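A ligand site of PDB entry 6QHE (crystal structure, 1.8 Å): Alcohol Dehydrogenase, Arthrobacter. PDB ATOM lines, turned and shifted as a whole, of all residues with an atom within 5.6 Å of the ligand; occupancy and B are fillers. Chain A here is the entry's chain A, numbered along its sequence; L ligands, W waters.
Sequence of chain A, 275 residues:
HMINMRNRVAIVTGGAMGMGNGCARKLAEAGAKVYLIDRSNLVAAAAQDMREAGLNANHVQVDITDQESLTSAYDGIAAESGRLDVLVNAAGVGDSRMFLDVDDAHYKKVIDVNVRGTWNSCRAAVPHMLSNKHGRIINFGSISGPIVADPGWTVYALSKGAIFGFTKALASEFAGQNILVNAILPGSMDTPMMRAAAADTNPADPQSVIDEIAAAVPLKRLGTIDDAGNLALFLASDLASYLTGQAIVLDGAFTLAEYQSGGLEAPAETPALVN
The backbone carbonyl oxygen of Asp 38 is in hydrogen-bond range of the backbone NH of Val 62, 3.0 Å away. OD1 of Asp 38 sits at hydrogen-bond distance from N of Ser 40 (2.9 Å). The backbone NH of Gly 15 lies within hydrogen-bond range of the side-chain carboxylate of Asp 38. N of Met 193 lies close to OG1 of Thr 191 (3.4 Å). The backbone NH (N) of Ala 90 is in hydrogen-bond range of the side-chain hydroxyl (OG1) of Thr 13 (3.1 Å). The side-chain carboxylate (OD1) of Asp 63 lies within hydrogen-bond range of the side-chain hydroxyl (OG1) of Thr 65, 2.6 Å away. N of Gly 14 sits at hydrogen-bond distance from O of Ile 37, at 2.9 Å. The backbone carbonyl oxygen (O) of Pro 186 lies within hydrogen-bond range of the backbone NH (N) of Ile 143 (3.3 Å).
Water W1 lies within hydrogen-bond range of O1 of the ligand and O of Gly 92. Water W2 lies within hydrogen-bond range of O of Ala 91 (2.7 Å), O12 of the ligand (2.8 Å) and O of Asn 89 (2.9 Å).
An oxygen (O14) of the ligand lies close to the backbone carbonyl oxygen (O) of Gly 187. Merely in contact with the ligand: Ala 90 (3.0 Å), Pro 192 (3.1 Å), Ser 142 (3.3 Å), Met 17 (3.3 Å), Gly 18 (3.3 Å), Gly 14 (3.3 Å), Gly 141 (3.3 Å), Met 194 (3.4 Å), Ala 91 (3.5 Å), Pro 186 (3.5 Å), Phe 140 (3.6 Å), Ala 16 (3.6 Å), Val 62 (3.7 Å), Val 113 (3.7 Å), Gly 92 (3.7 Å), Ser 40 (3.8 Å) and Ser 188 (3.95 Å). 28 residues have an atom within 4 Å of the ligand: Gly 14, Ala 16, Met 17, Gly 18, Met 19, Asp 38, Arg 39, Ser 40, Val 62, Asp 63, Ile 64, Ala 90, Ala 91, Gly 92, Val 113, Phe 140, Gly 141, Ser 142, Tyr 156, Lys 160, Pro 186, Gly 187, Ser 188, Met 189, Thr 191, Pro 192, Met 193 and Met 194.
OD1 of Asp 38 sits at hydrogen-bond distance from O6 of the ligand, at 2.4 Å. An oxygen (O9) of the ligand sits at hydrogen-bond distance from the backbone NH (N) of Met 19, 2.6 Å away. O8 of the ligand lies within hydrogen-bond range of OG1 of Thr 191. The side-chain hydroxyl (OH) of Tyr 156 is in hydrogen-bond range of an oxygen (O13) of the ligand, at 2.7 Å. The side-chain amino group (NZ) of Lys 160 lies within hydrogen-bond range of an oxygen (O12) of the ligand. An oxygen (O14) of the ligand is in hydrogen-bond range of the backbone NH (N) of Met 189. OD1 of Asp 63 is in hydrogen-bond range of N3 of the ligand. The backbone NH (N) of Met 193 sits at hydrogen-bond distance from an oxygen (O2) of the ligand (3.3 Å). The backbone NH (N) of Arg 39 lies close to a nitrogen (N5) of the ligand. The backbone NH (N) of Ile 64 is in hydrogen-bond range of a nitrogen (N4) of the ligand (3.3 Å).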
ATOM      1  N   THR A  13      -1.636 -16.107 -13.538  1.00  0.00           N
ATOM      2  CA  THR A  13      -1.556 -17.271 -12.613  1.00  0.00           C
ATOM      3  C   THR A  13      -0.081 -17.563 -12.367  1.00  0.00           C
ATOM      4  O   THR A  13       0.738 -17.304 -13.259  1.00  0.00           O
ATOM      5  CB  THR A  13      -2.357 -18.489 -13.087  1.00  0.00           C
ATOM      6  OG1 THR A  13      -1.589 -19.137 -14.107  1.00  0.00           O
ATOM      7  CG2 THR A  13      -3.758 -18.122 -13.561  1.00  0.00           C
ATOM      8  N   GLY A  14       0.243 -18.096 -11.203  1.00  0.00           N
ATOM      9  CA  GLY A  14       1.642 -18.326 -10.791  1.00  0.00           C
ATOM     10  C   GLY A  14       2.357 -17.008 -10.503  1.00  0.00           C
ATOM     11  O   GLY A  14       3.567 -16.975 -10.579  1.00  0.00           O
ATOM     12  N   GLY A  15       1.615 -15.940 -10.184  1.00  0.00           N
ATOM     13  CA  GLY A  15       2.165 -14.587 -10.042  1.00  0.00           C
ATOM     14  C   GLY A  15       3.108 -14.397  -8.846  1.00  0.00           C
ATOM     15  O   GLY A  15       3.807 -13.393  -8.833  1.00  0.00           O
ATOM     16  N   ALA A  16       3.131 -15.317  -7.875  1.00  0.00           N
ATOM     17  CA  ALA A  16       3.871 -15.104  -6.597  1.00  0.00           C
ATOM     18  C   ALA A  16       5.381 -15.173  -6.854  1.00  0.00           C
ATOM     19  O   ALA A  16       6.124 -14.500  -6.143  1.00  0.00           O
ATOM     20  CB  ALA A  16       3.476 -16.121  -5.556  1.00  0.00           C
ATOM     21  N   MET A  17       5.833 -15.990  -7.805  1.00  0.00           N
ATOM     22  CA  MET A  17       7.270 -16.179  -8.053  1.00  0.00           C
ATOM     23  C   MET A  17       7.512 -16.703  -9.472  1.00  0.00           C
ATOM     24  O   MET A  17       6.526 -16.942 -10.183  1.00  0.00           O
ATOM     25  CB  MET A  17       7.859 -17.187  -7.047  1.00  0.00           C
ATOM     26  CG  MET A  17       7.351 -18.583  -7.241  1.00  0.00           C
ATOM     27  SD  MET A  17       7.699 -19.695  -5.845  1.00  0.00           S
ATOM     28  CE  MET A  17       6.508 -19.061  -4.674  1.00  0.00           C
ATOM     29  N   GLY A  18       8.767 -16.869  -9.837  1.00  0.00           N
ATOM     30  CA  GLY A  18       9.136 -17.480 -11.125  1.00  0.00           C
ATOM     31  C   GLY A  18       8.598 -16.698 -12.302  1.00  0.00           C
ATOM     32  O   GLY A  18       8.440 -15.459 -12.205  1.00  0.00           O
ATOM     33  N   MET A  19       8.345 -17.390 -13.414  1.00  0.00           N
ATOM     34  CA  MET A  19       8.012 -16.674 -14.664  1.00  0.00           C
ATOM     35  C   MET A  19       6.687 -15.911 -14.542  1.00  0.00           C
ATOM     36  O   MET A  19       6.553 -14.847 -15.149  1.00  0.00           O
ATOM     37  CB  MET A  19       8.028 -17.632 -15.845  1.00  0.00           C
ATOM     38  CG  MET A  19       9.470 -18.011 -16.159  1.00  0.00           C
ATOM     39  SD  MET A  19       9.669 -19.072 -17.621  1.00  0.00           S
ATOM     40  CE  MET A  19       9.160 -20.642 -16.993  1.00  0.00           C
ATOM     41  N   GLY A  20       5.712 -16.430 -13.804  1.00  0.00           N
ATOM     42  CA  GLY A  20       4.450 -15.677 -13.601  1.00  0.00           C
ATOM     43  C   GLY A  20       4.721 -14.329 -12.952  1.00  0.00           C
ATOM     44  O   GLY A  20       4.172 -13.323 -13.387  1.00  0.00           O
ATOM     45  N   ILE A  37      -2.496 -14.193  -9.338  1.00  0.00           N
ATOM     46  CA  ILE A  37      -3.319 -15.355  -8.905  1.00  0.00           C
ATOM     47  C   ILE A  37      -2.319 -16.439  -8.502  1.00  0.00           C
ATOM     48  O   ILE A  37      -1.468 -16.814  -9.300  1.00  0.00           O
ATOM     49  CB  ILE A  37      -4.346 -15.795  -9.970  1.00  0.00           C
ATOM     50  CG1 ILE A  37      -5.616 -14.930  -9.936  1.00  0.00           C
ATOM     51  CG2 ILE A  37      -4.700 -17.265  -9.850  1.00  0.00           C
ATOM     52  CD1 ILE A  37      -5.405 -13.452  -9.839  1.00  0.00           C
ATOM     53  N   ASP A  38      -2.417 -16.938  -7.276  1.00  0.00           N
ATOM     54  CA  ASP A  38      -1.491 -17.976  -6.802  1.00  0.00           C
ATOM     55  C   ASP A  38      -2.082 -18.641  -5.550  1.00  0.00           C
ATOM     56  O   ASP A  38      -2.826 -17.965  -4.788  1.00  0.00           O
ATOM     57  CB  ASP A  38      -0.134 -17.343  -6.527  1.00  0.00           C
ATOM     58  CG  ASP A  38       1.037 -18.285  -6.712  1.00  0.00           C
ATOM     59  OD1 ASP A  38       1.109 -19.303  -5.931  1.00  0.00           O
ATOM     60  OD2 ASP A  38       1.867 -18.032  -7.632  1.00  0.00           O
ATOM     61  N   ARG A  39      -1.774 -19.911  -5.367  1.00  0.00           N
ATOM     62  CA  ARG A  39      -2.145 -20.654  -4.125  1.00  0.00           C
ATOM     63  C   ARG A  39      -1.190 -20.247  -3.004  1.00  0.00           C
ATOM     64  O   ARG A  39      -1.537 -20.455  -1.858  1.00  0.00           O
ATOM     65  CB  ARG A  39      -2.139 -22.166  -4.395  1.00  0.00           C
ATOM     66  CG  ARG A  39      -0.764 -22.823  -4.564  1.00  0.00           C
ATOM     67  N   SER A  40      -0.002 -19.734  -3.323  1.00  0.00           N
ATOM     68  CA  SER A  40       1.062 -19.465  -2.327  1.00  0.00           C
ATOM     69  C   SER A  40       0.634 -18.333  -1.371  1.00  0.00           C
ATOM     70  O   SER A  40       0.119 -17.299  -1.831  1.00  0.00           O
ATOM     71  CB  SER A  40       2.354 -19.115  -3.008  1.00  0.00           C
ATOM     72  OG  SER A  40       3.323 -18.641  -2.114  1.00  0.00           O
ATOM     73  N   VAL A  62      -5.807 -18.153  -4.526  1.00  0.00           N
ATOM     74  CA  VAL A  62      -6.824 -19.131  -4.991  1.00  0.00           C
ATOM     75  C   VAL A  62      -6.085 -20.277  -5.697  1.00  0.00           C
ATOM     76  O   VAL A  62      -4.973 -20.029  -6.248  1.00  0.00           O
ATOM     77  CB  VAL A  62      -7.843 -18.417  -5.887  1.00  0.00           C
ATOM     78  CG1 VAL A  62      -7.204 -17.782  -7.114  1.00  0.00           C
ATOM     79  CG2 VAL A  62      -8.978 -19.331  -6.268  1.00  0.00           C
ATOM     80  N   ASP A  63      -6.659 -21.457  -5.646  1.00  0.00           N
ATOM     81  CA  ASP A  63      -6.130 -22.675  -6.285  1.00  0.00           C
ATOM     82  C   ASP A  63      -6.797 -22.816  -7.660  1.00  0.00           C
ATOM     83  O   ASP A  63      -8.011 -22.976  -7.733  1.00  0.00           O
ATOM     84  CB  ASP A  63      -6.325 -23.902  -5.395  1.00  0.00           C
ATOM     85  CG  ASP A  63      -5.566 -25.109  -5.917  1.00  0.00           C
ATOM     86  OD1 ASP A  63      -5.552 -25.322  -7.141  1.00  0.00           O
ATOM     87  OD2 ASP A  63      -4.912 -25.788  -5.110  1.00  0.00           O
ATOM     88  N   ILE A  64      -6.019 -22.780  -8.749  1.00  0.00           N
ATOM     89  CA  ILE A  64      -6.592 -22.829 -10.130  1.00  0.00           C
ATOM     90  C   ILE A  64      -7.245 -24.191 -10.386  1.00  0.00           C
ATOM     91  O   ILE A  64      -7.990 -24.275 -11.367  1.00  0.00           O
ATOM     92  CB  ILE A  64      -5.521 -22.499 -11.184  1.00  0.00           C
ATOM     93  CG1 ILE A  64      -4.368 -23.507 -11.154  1.00  0.00           C
ATOM     94  CG2 ILE A  64      -5.029 -21.075 -10.980  1.00  0.00           C
ATOM     95  CD1 ILE A  64      -3.337 -23.296 -12.295  1.00  0.00           C
ATOM     96  N   THR A  65      -6.975 -25.235  -9.601  1.00  0.00           N
ATOM     97  CA  THR A  65      -7.627 -26.560  -9.777  1.00  0.00           C
ATOM     98  C   THR A  65      -9.041 -26.562  -9.153  1.00  0.00           C
ATOM     99  O   THR A  65      -9.749 -27.532  -9.372  1.00  0.00           O
ATOM    100  CB  THR A  65      -6.788 -27.708  -9.203  1.00  0.00           C
ATOM    101  OG1 THR A  65      -6.739 -27.584  -7.784  1.00  0.00           O
ATOM    102  CG2 THR A  65      -5.368 -27.737  -9.765  1.00  0.00           C
ATOM    103  N   ASN A  89      -1.201 -17.778 -18.157  1.00  0.00           N
ATOM    104  CA  ASN A  89      -1.298 -19.042 -17.386  1.00  0.00           C
ATOM    105  C   ASN A  89       0.116 -19.556 -17.115  1.00  0.00           C
ATOM    106  O   ASN A  89       0.599 -20.407 -17.883  1.00  0.00           O
ATOM    107  CB  ASN A  89      -2.147 -20.074 -18.136  1.00  0.00           C
ATOM    108  CG  ASN A  89      -3.609 -19.688 -18.180  1.00  0.00           C
ATOM    109  OD1 ASN A  89      -4.175 -19.591 -19.252  1.00  0.00           O
ATOM    110  ND2 ASN A  89      -4.193 -19.400 -17.045  1.00  0.00           N
ATOM    111  N   ALA A  90       0.766 -19.041 -16.077  1.00  0.00           N
ATOM    112  CA  ALA A  90       2.167 -19.406 -15.756  1.00  0.00           C
ATOM    113  C   ALA A  90       2.211 -20.399 -14.587  1.00  0.00           C
ATOM    114  O   ALA A  90       3.229 -21.006 -14.390  1.00  0.00           O
ATOM    115  CB  ALA A  90       2.968 -18.169 -15.494  1.00  0.00           C
ATOM    116  N   ALA A  91       1.124 -20.602 -13.851  1.00  0.00           N
ATOM    117  CA  ALA A  91       1.134 -21.562 -12.734  1.00  0.00           C
ATOM    118  C   ALA A  91       1.420 -22.956 -13.263  1.00  0.00           C
ATOM    119  O   ALA A  91       0.765 -23.381 -14.267  1.00  0.00           O
ATOM    120  CB  ALA A  91      -0.191 -21.551 -12.014  1.00  0.00           C
ATOM    121  N   GLY A  92       2.324 -23.705 -12.631  1.00  0.00           N
ATOM    122  CA  GLY A  92       2.668 -25.044 -13.116  1.00  0.00           C
ATOM    123  C   GLY A  92       3.453 -25.794 -12.071  1.00  0.00           C
ATOM    124  O   GLY A  92       3.958 -25.138 -11.108  1.00  0.00           O
ATOM    125  N   VAL A  93       3.528 -27.099 -12.218  1.00  0.00           N
ATOM    126  CA  VAL A  93       4.429 -27.955 -11.411  1.00  0.00           C
ATOM    127  C   VAL A  93       5.316 -28.764 -12.342  1.00  0.00           C
ATOM    128  O   VAL A  93       4.864 -29.127 -13.458  1.00  0.00           O
ATOM    129  CB  VAL A  93       3.636 -28.835 -10.429  1.00  0.00           C
ATOM    130  CG1 VAL A  93       2.834 -28.003  -9.439  1.00  0.00           C
ATOM    131  CG2 VAL A  93       2.719 -29.793 -11.122  1.00  0.00           C
ATOM    132  N   GLY A  94       6.547 -29.031 -11.898  1.00  0.00           N
ATOM    133  CA  GLY A  94       7.610 -29.592 -12.729  1.00  0.00           C
ATOM    134  C   GLY A  94       8.118 -30.923 -12.218  1.00  0.00           C
ATOM    135  O   GLY A  94       9.253 -31.225 -12.434  1.00  0.00           O
ATOM    136  N   VAL A 113      -2.829 -29.511 -12.231  1.00  0.00           N
ATOM    137  CA  VAL A 113      -2.317 -28.105 -12.190  1.00  0.00           C
ATOM    138  C   VAL A 113      -2.026 -27.622 -13.624  1.00  0.00           C
ATOM    139  O   VAL A 113      -2.500 -26.546 -14.013  1.00  0.00           O
ATOM    140  CB  VAL A 113      -1.088 -27.974 -11.288  1.00  0.00           C
ATOM    141  CG1 VAL A 113      -0.559 -26.560 -11.352  1.00  0.00           C
ATOM    142  CG2 VAL A 113      -1.398 -28.384  -9.855  1.00  0.00           C
ATOM    143  N   ASN A 114      -1.236 -28.391 -14.360  1.00  0.00           N
ATOM    144  CA  ASN A 114      -0.688 -27.940 -15.668  1.00  0.00           C
ATOM    145  C   ASN A 114      -1.796 -27.858 -16.712  1.00  0.00           C
ATOM    146  O   ASN A 114      -1.782 -26.921 -17.520  1.00  0.00           O
ATOM    147  CB  ASN A 114       0.484 -28.813 -16.129  1.00  0.00           C
ATOM    148  CG  ASN A 114       1.717 -28.621 -15.261  1.00  0.00           C
ATOM    149  OD1 ASN A 114       1.681 -27.832 -14.301  1.00  0.00           O
ATOM    150  ND2 ASN A 114       2.795 -29.329 -15.586  1.00  0.00           N
ATOM    151  N   PHE A 140       1.649 -21.116 -20.790  1.00  0.00           N
ATOM    152  CA  PHE A 140       3.028 -21.647 -20.658  1.00  0.00           C
ATOM    153  C   PHE A 140       3.033 -23.137 -20.934  1.00  0.00           C
ATOM    154  O   PHE A 140       2.441 -23.952 -20.184  1.00  0.00           O
ATOM    155  CB  PHE A 140       3.623 -21.283 -19.293  1.00  0.00           C
ATOM    156  CG  PHE A 140       4.261 -19.920 -19.283  1.00  0.00           C
ATOM    157  CD1 PHE A 140       3.505 -18.760 -19.317  1.00  0.00           C
ATOM    158  CD2 PHE A 140       5.645 -19.810 -19.245  1.00  0.00           C
ATOM    159  CE1 PHE A 140       4.111 -17.516 -19.336  1.00  0.00           C
ATOM    160  CE2 PHE A 140       6.246 -18.564 -19.278  1.00  0.00           C
ATOM    161  CZ  PHE A 140       5.483 -17.423 -19.310  1.00  0.00           C
ATOM    162  N   GLY A 141       3.671 -23.500 -22.043  1.00  0.00           N
ATOM    163  CA  GLY A 141       4.012 -24.889 -22.334  1.00  0.00           C
ATOM    164  C   GLY A 141       5.416 -25.168 -21.823  1.00  0.00           C
ATOM    165  O   GLY A 141       5.772 -24.715 -20.752  1.00  0.00           O
ATOM    166  N   SER A 142       6.166 -25.912 -22.601  1.00  0.00           N
ATOM    167  CA  SER A 142       7.593 -26.208 -22.382  1.00  0.00           C
ATOM    168  C   SER A 142       8.141 -26.699 -23.705  1.00  0.00           C
ATOM    169  O   SER A 142       7.340 -27.226 -24.524  1.00  0.00           O
ATOM    170  CB  SER A 142       7.780 -27.276 -21.308  1.00  0.00           C
ATOM    171  OG  SER A 142       9.165 -27.592 -21.166  1.00  0.00           O
ATOM    172  N   ILE A 143       9.461 -26.641 -23.876  1.00  0.00           N
ATOM    173  CA  ILE A 143      10.127 -27.413 -24.952  1.00  0.00           C
ATOM    174  C   ILE A 143       9.910 -28.921 -24.707  1.00  0.00           C
ATOM    175  O   ILE A 143       9.919 -29.690 -25.693  1.00  0.00           O
ATOM    176  CB  ILE A 143      11.591 -27.033 -25.095  1.00  0.00           C
ATOM    177  CG1 ILE A 143      12.371 -27.268 -23.792  1.00  0.00           C
ATOM    178  CG2 ILE A 143      11.682 -25.589 -25.602  1.00  0.00           C
ATOM    179  CD1 ILE A 143      13.860 -27.172 -23.994  1.00  0.00           C
ATOM    180  N   TYR A 156       4.931 -34.799 -17.197  1.00  0.00           N
ATOM    181  CA  TYR A 156       5.130 -33.363 -17.487  1.00  0.00           C
ATOM    182  C   TYR A 156       5.013 -33.130 -18.998  1.00  0.00           C
ATOM    183  O   TYR A 156       4.292 -32.182 -19.409  1.00  0.00           O
ATOM    184  CB  TYR A 156       6.488 -32.919 -16.964  1.00  0.00           C
ATOM    185  CG  TYR A 156       6.760 -31.451 -17.136  1.00  0.00           C
ATOM    186  CD1 TYR A 156       6.254 -30.509 -16.266  1.00  0.00           C
ATOM    187  CD2 TYR A 156       7.590 -30.998 -18.143  1.00  0.00           C
ATOM    188  CE1 TYR A 156       6.520 -29.166 -16.402  1.00  0.00           C
ATOM    189  CE2 TYR A 156       7.905 -29.654 -18.283  1.00  0.00           C
ATOM    190  CZ  TYR A 156       7.370 -28.733 -17.419  1.00  0.00           C
ATOM    191  OH  TYR A 156       7.622 -27.408 -17.589  1.00  0.00           O
ATOM    192  N   LYS A 160       2.387 -30.780 -21.103  1.00  0.00           N
ATOM    193  CA  LYS A 160       2.803 -29.595 -21.923  1.00  0.00           C
ATOM    194  C   LYS A 160       2.421 -29.836 -23.398  1.00  0.00           C
ATOM    195  O   LYS A 160       2.131 -28.854 -24.090  1.00  0.00           O
ATOM    196  CB  LYS A 160       4.287 -29.307 -21.678  1.00  0.00           C
ATOM    197  CG  LYS A 160       4.608 -28.902 -20.240  1.00  0.00           C
ATOM    198  CD  LYS A 160       3.713 -27.783 -19.749  1.00  0.00           C
ATOM    199  CE  LYS A 160       4.200 -27.089 -18.485  1.00  0.00           C
ATOM    200  NZ  LYS A 160       3.424 -25.859 -18.214  1.00  0.00           N
ATOM    201  N   PRO A 186       9.268 -22.240 -22.895  1.00  0.00           N
ATOM    202  CA  PRO A 186      10.569 -21.891 -22.351  1.00  0.00           C
ATOM    203  C   PRO A 186      11.528 -23.096 -22.417  1.00  0.00           C
ATOM    204  O   PRO A 186      11.095 -24.278 -22.346  1.00  0.00           O
ATOM    205  CB  PRO A 186      10.289 -21.541 -20.865  1.00  0.00           C
ATOM    206  CG  PRO A 186       8.798 -21.374 -20.796  1.00  0.00           C
ATOM    207  CD  PRO A 186       8.239 -22.327 -21.835  1.00  0.00           C
ATOM    208  N   GLY A 187      12.817 -22.794 -22.521  1.00  0.00           N
ATOM    209  CA  GLY A 187      13.879 -23.776 -22.324  1.00  0.00           C
ATOM    210  C   GLY A 187      14.283 -23.772 -20.866  1.00  0.00           C
ATOM    211  O   GLY A 187      13.387 -23.793 -19.966  1.00  0.00           O
ATOM    212  N   SER A 188      15.574 -23.738 -20.584  1.00  0.00           N
ATOM    213  CA  SER A 188      16.110 -23.770 -19.188  1.00  0.00           C
ATOM    214  C   SER A 188      16.080 -22.378 -18.585  1.00  0.00           C
ATOM    215  O   SER A 188      16.850 -21.542 -19.044  1.00  0.00           O
ATOM    216  CB  SER A 188      17.490 -24.344 -19.222  1.00  0.00           C
ATOM    217  OG  SER A 188      17.469 -25.667 -19.761  1.00  0.00           O
ATOM    218  N   MET A 189      15.173 -22.113 -17.653  1.00  0.00           N
ATOM    219  CA  MET A 189      14.938 -20.780 -17.082  1.00  0.00           C
ATOM    220  C   MET A 189      15.325 -20.777 -15.586  1.00  0.00           C
ATOM    221  O   MET A 189      15.097 -21.778 -14.921  1.00  0.00           O
ATOM    222  CB  MET A 189      13.480 -20.336 -17.213  1.00  0.00           C
ATOM    223  CG  MET A 189      12.902 -20.633 -18.608  1.00  0.00           C
ATOM    224  SD  MET A 189      13.744 -19.831 -19.991  1.00  0.00           S
ATOM    225  CE  MET A 189      13.030 -18.195 -19.927  1.00  0.00           C
ATOM    226  N   ASP A 190      15.856 -19.654 -15.106  1.00  0.00           N
ATOM    227  CA  ASP A 190      16.309 -19.511 -13.692  1.00  0.00           C
ATOM    228  C   ASP A 190      15.126 -19.157 -12.796  1.00  0.00           C
ATOM    229  O   ASP A 190      14.845 -17.960 -12.615  1.00  0.00           O
ATOM    230  CB  ASP A 190      17.438 -18.514 -13.582  1.00  0.00           C
ATOM    231  CG  ASP A 190      18.116 -18.605 -12.217  1.00  0.00           C
ATOM    232  OD1 ASP A 190      17.641 -19.386 -11.366  1.00  0.00           O
ATOM    233  OD2 ASP A 190      19.108 -17.916 -12.037  1.00  0.00           O
ATOM    234  N   THR A 191      14.443 -20.177 -12.297  1.00  0.00           N
ATOM    235  CA  THR A 191      13.234 -20.021 -11.456  1.00  0.00           C
ATOM    236  C   THR A 191      13.371 -20.884 -10.204  1.00  0.00           C
ATOM    237  O   THR A 191      14.213 -21.787 -10.172  1.00  0.00           O
ATOM    238  CB  THR A 191      11.964 -20.450 -12.210  1.00  0.00           C
ATOM    239  OG1 THR A 191      12.055 -21.843 -12.441  1.00  0.00           O
ATOM    240  CG2 THR A 191      11.806 -19.712 -13.519  1.00  0.00           C
ATOM    241  N   PRO A 192      12.500 -20.671  -9.193  1.00  0.00           N
ATOM    242  CA  PRO A 192      12.412 -21.602  -8.065  1.00  0.00           C
ATOM    243  C   PRO A 192      12.250 -23.066  -8.486  1.00  0.00           C
ATOM    244  O   PRO A 192      12.944 -23.909  -7.955  1.00  0.00           O
ATOM    245  CB  PRO A 192      11.205 -21.081  -7.258  1.00  0.00           C
ATOM    246  CG  PRO A 192      11.183 -19.589  -7.578  1.00  0.00           C
ATOM    247  CD  PRO A 192      11.628 -19.495  -9.034  1.00  0.00           C
ATOM    248  N   MET A 193      11.402 -23.347  -9.484  1.00  0.00           N
ATOM    249  CA  MET A 193      11.202 -24.736  -9.989  1.00  0.00           C
ATOM    250  C   MET A 193      12.537 -25.310 -10.486  1.00  0.00           C
ATOM    251  O   MET A 193      12.863 -26.436 -10.120  1.00  0.00           O
ATOM    252  CB  MET A 193      10.152 -24.759 -11.119  1.00  0.00           C
ATOM    253  CG  MET A 193       9.865 -26.149 -11.690  1.00  0.00           C
ATOM    254  SD  MET A 193       8.744 -26.068 -13.163  1.00  0.00           S
ATOM    255  CE  MET A 193       7.219 -25.561 -12.385  1.00  0.00           C
ATOM    256  N   MET A 194      13.314 -24.562 -11.261  1.00  0.00           N
ATOM    257  CA  MET A 194      14.618 -25.040 -11.812  1.00  0.00           C
ATOM    258  C   MET A 194      15.610 -25.208 -10.662  1.00  0.00           C
ATOM    259  O   MET A 194      16.342 -26.220 -10.659  1.00  0.00           O
ATOM    260  CB  MET A 194      15.166 -24.031 -12.838  1.00  0.00           C
ATOM    261  CG  MET A 194      16.566 -24.307 -13.332  1.00  0.00           C
ATOM    262  SD  MET A 194      16.724 -25.857 -14.245  1.00  0.00           S
ATOM    263  CE  MET A 194      15.758 -25.482 -15.713  1.00  0.00           C
HETATM  264  P1  LIG L   1       7.778 -21.737 -10.245  1.00  0.00           P
HETATM  265  O1  LIG L   1       7.465 -23.046  -9.524  1.00  0.00           O
HETATM  266  O2  LIG L   1       9.120 -21.089 -10.001  1.00  0.00           O
HETATM  267  O3  LIG L   1       6.554 -20.721 -10.086  1.00  0.00           O
HETATM  268  C1  LIG L   1       5.242 -21.396 -10.214  1.00  0.00           C
HETATM  269  C2  LIG L   1       4.187 -20.567  -9.536  1.00  0.00           C
HETATM  270  O4  LIG L   1       2.917 -21.225  -9.795  1.00  0.00           O
HETATM  271  C3  LIG L   1       4.310 -20.411  -7.998  1.00  0.00           C
HETATM  272  O5  LIG L   1       4.125 -19.046  -7.611  1.00  0.00           O
HETATM  273  C4  LIG L   1       3.243 -21.393  -7.467  1.00  0.00           C
HETATM  274  O6  LIG L   1       2.707 -21.104  -6.183  1.00  0.00           O
HETATM  275  C5  LIG L   1       2.198 -21.255  -8.576  1.00  0.00           C
HETATM  276  N1  LIG L   1       1.235 -22.334  -8.584  1.00  0.00           N
HETATM  277  C6  LIG L   1       1.543 -23.693  -8.600  1.00  0.00           C
HETATM  278  N2  LIG L   1       0.477 -24.454  -8.498  1.00  0.00           N
HETATM  279  C7  LIG L   1      -0.602 -23.556  -8.421  1.00  0.00           C
HETATM  280  C8  LIG L   1      -2.003 -23.745  -8.285  1.00  0.00           C
HETATM  281  N3  LIG L   1      -2.570 -24.945  -8.163  1.00  0.00           N
HETATM  282  N4  LIG L   1      -2.792 -22.636  -8.135  1.00  0.00           N
HETATM  283  C9  LIG L   1      -2.205 -21.412  -8.256  1.00  0.00           C
HETATM  284  N5  LIG L   1      -0.916 -21.102  -8.405  1.00  0.00           N
HETATM  285  C10 LIG L   1      -0.146 -22.229  -8.450  1.00  0.00           C
HETATM  286  O7  LIG L   1       7.645 -22.098 -11.830  1.00  0.00           O
HETATM  287  P2  LIG L   1       8.201 -21.336 -13.127  1.00  0.00           P
HETATM  288  O8  LIG L   1       9.567 -21.960 -13.351  1.00  0.00           O
HETATM  289  O9  LIG L   1       7.951 -19.897 -13.020  1.00  0.00           O
HETATM  290  O10 LIG L   1       7.195 -22.087 -14.192  1.00  0.00           O
HETATM  291  C11 LIG L   1       6.129 -21.371 -14.856  1.00  0.00           C
HETATM  292  C12 LIG L   1       5.622 -22.191 -16.025  1.00  0.00           C
HETATM  293  O11 LIG L   1       6.681 -22.382 -17.024  1.00  0.00           O
HETATM  294  C13 LIG L   1       5.133 -23.591 -15.655  1.00  0.00           C
HETATM  295  O12 LIG L   1       3.974 -23.881 -16.409  1.00  0.00           O
HETATM  296  C14 LIG L   1       6.350 -24.442 -15.994  1.00  0.00           C
HETATM  297  O13 LIG L   1       5.968 -25.788 -16.141  1.00  0.00           O
HETATM  298  C15 LIG L   1       6.814 -23.773 -17.295  1.00  0.00           C
HETATM  299  N6  LIG L   1       8.239 -24.094 -17.649  1.00  0.00           N
HETATM  300  C16 LIG L   1       9.285 -23.930 -16.725  1.00  0.00           C
HETATM  301  C17 LIG L   1      10.619 -24.079 -17.173  1.00  0.00           C
HETATM  302  C18 LIG L   1      11.789 -23.659 -16.334  1.00  0.00           C
HETATM  303  O14 LIG L   1      12.937 -23.913 -16.741  1.00  0.00           O
HETATM  304  N7  LIG L   1      11.519 -23.106 -15.160  1.00  0.00           N
HETATM  305  C19 LIG L   1      10.842 -24.703 -18.404  1.00  0.00           C
HETATM  306  C20 LIG L   1       9.788 -25.060 -19.191  1.00  0.00           C
HETATM  307  C21 LIG L   1       8.538 -24.553 -18.887  1.00  0.00           C
HETATM  308  O   HOH W   1       5.693 -24.799  -9.309  1.00  0.00           O
HETATM  309  O   HOH W   2       1.312 -22.990 -16.871  1.00  0.00           O
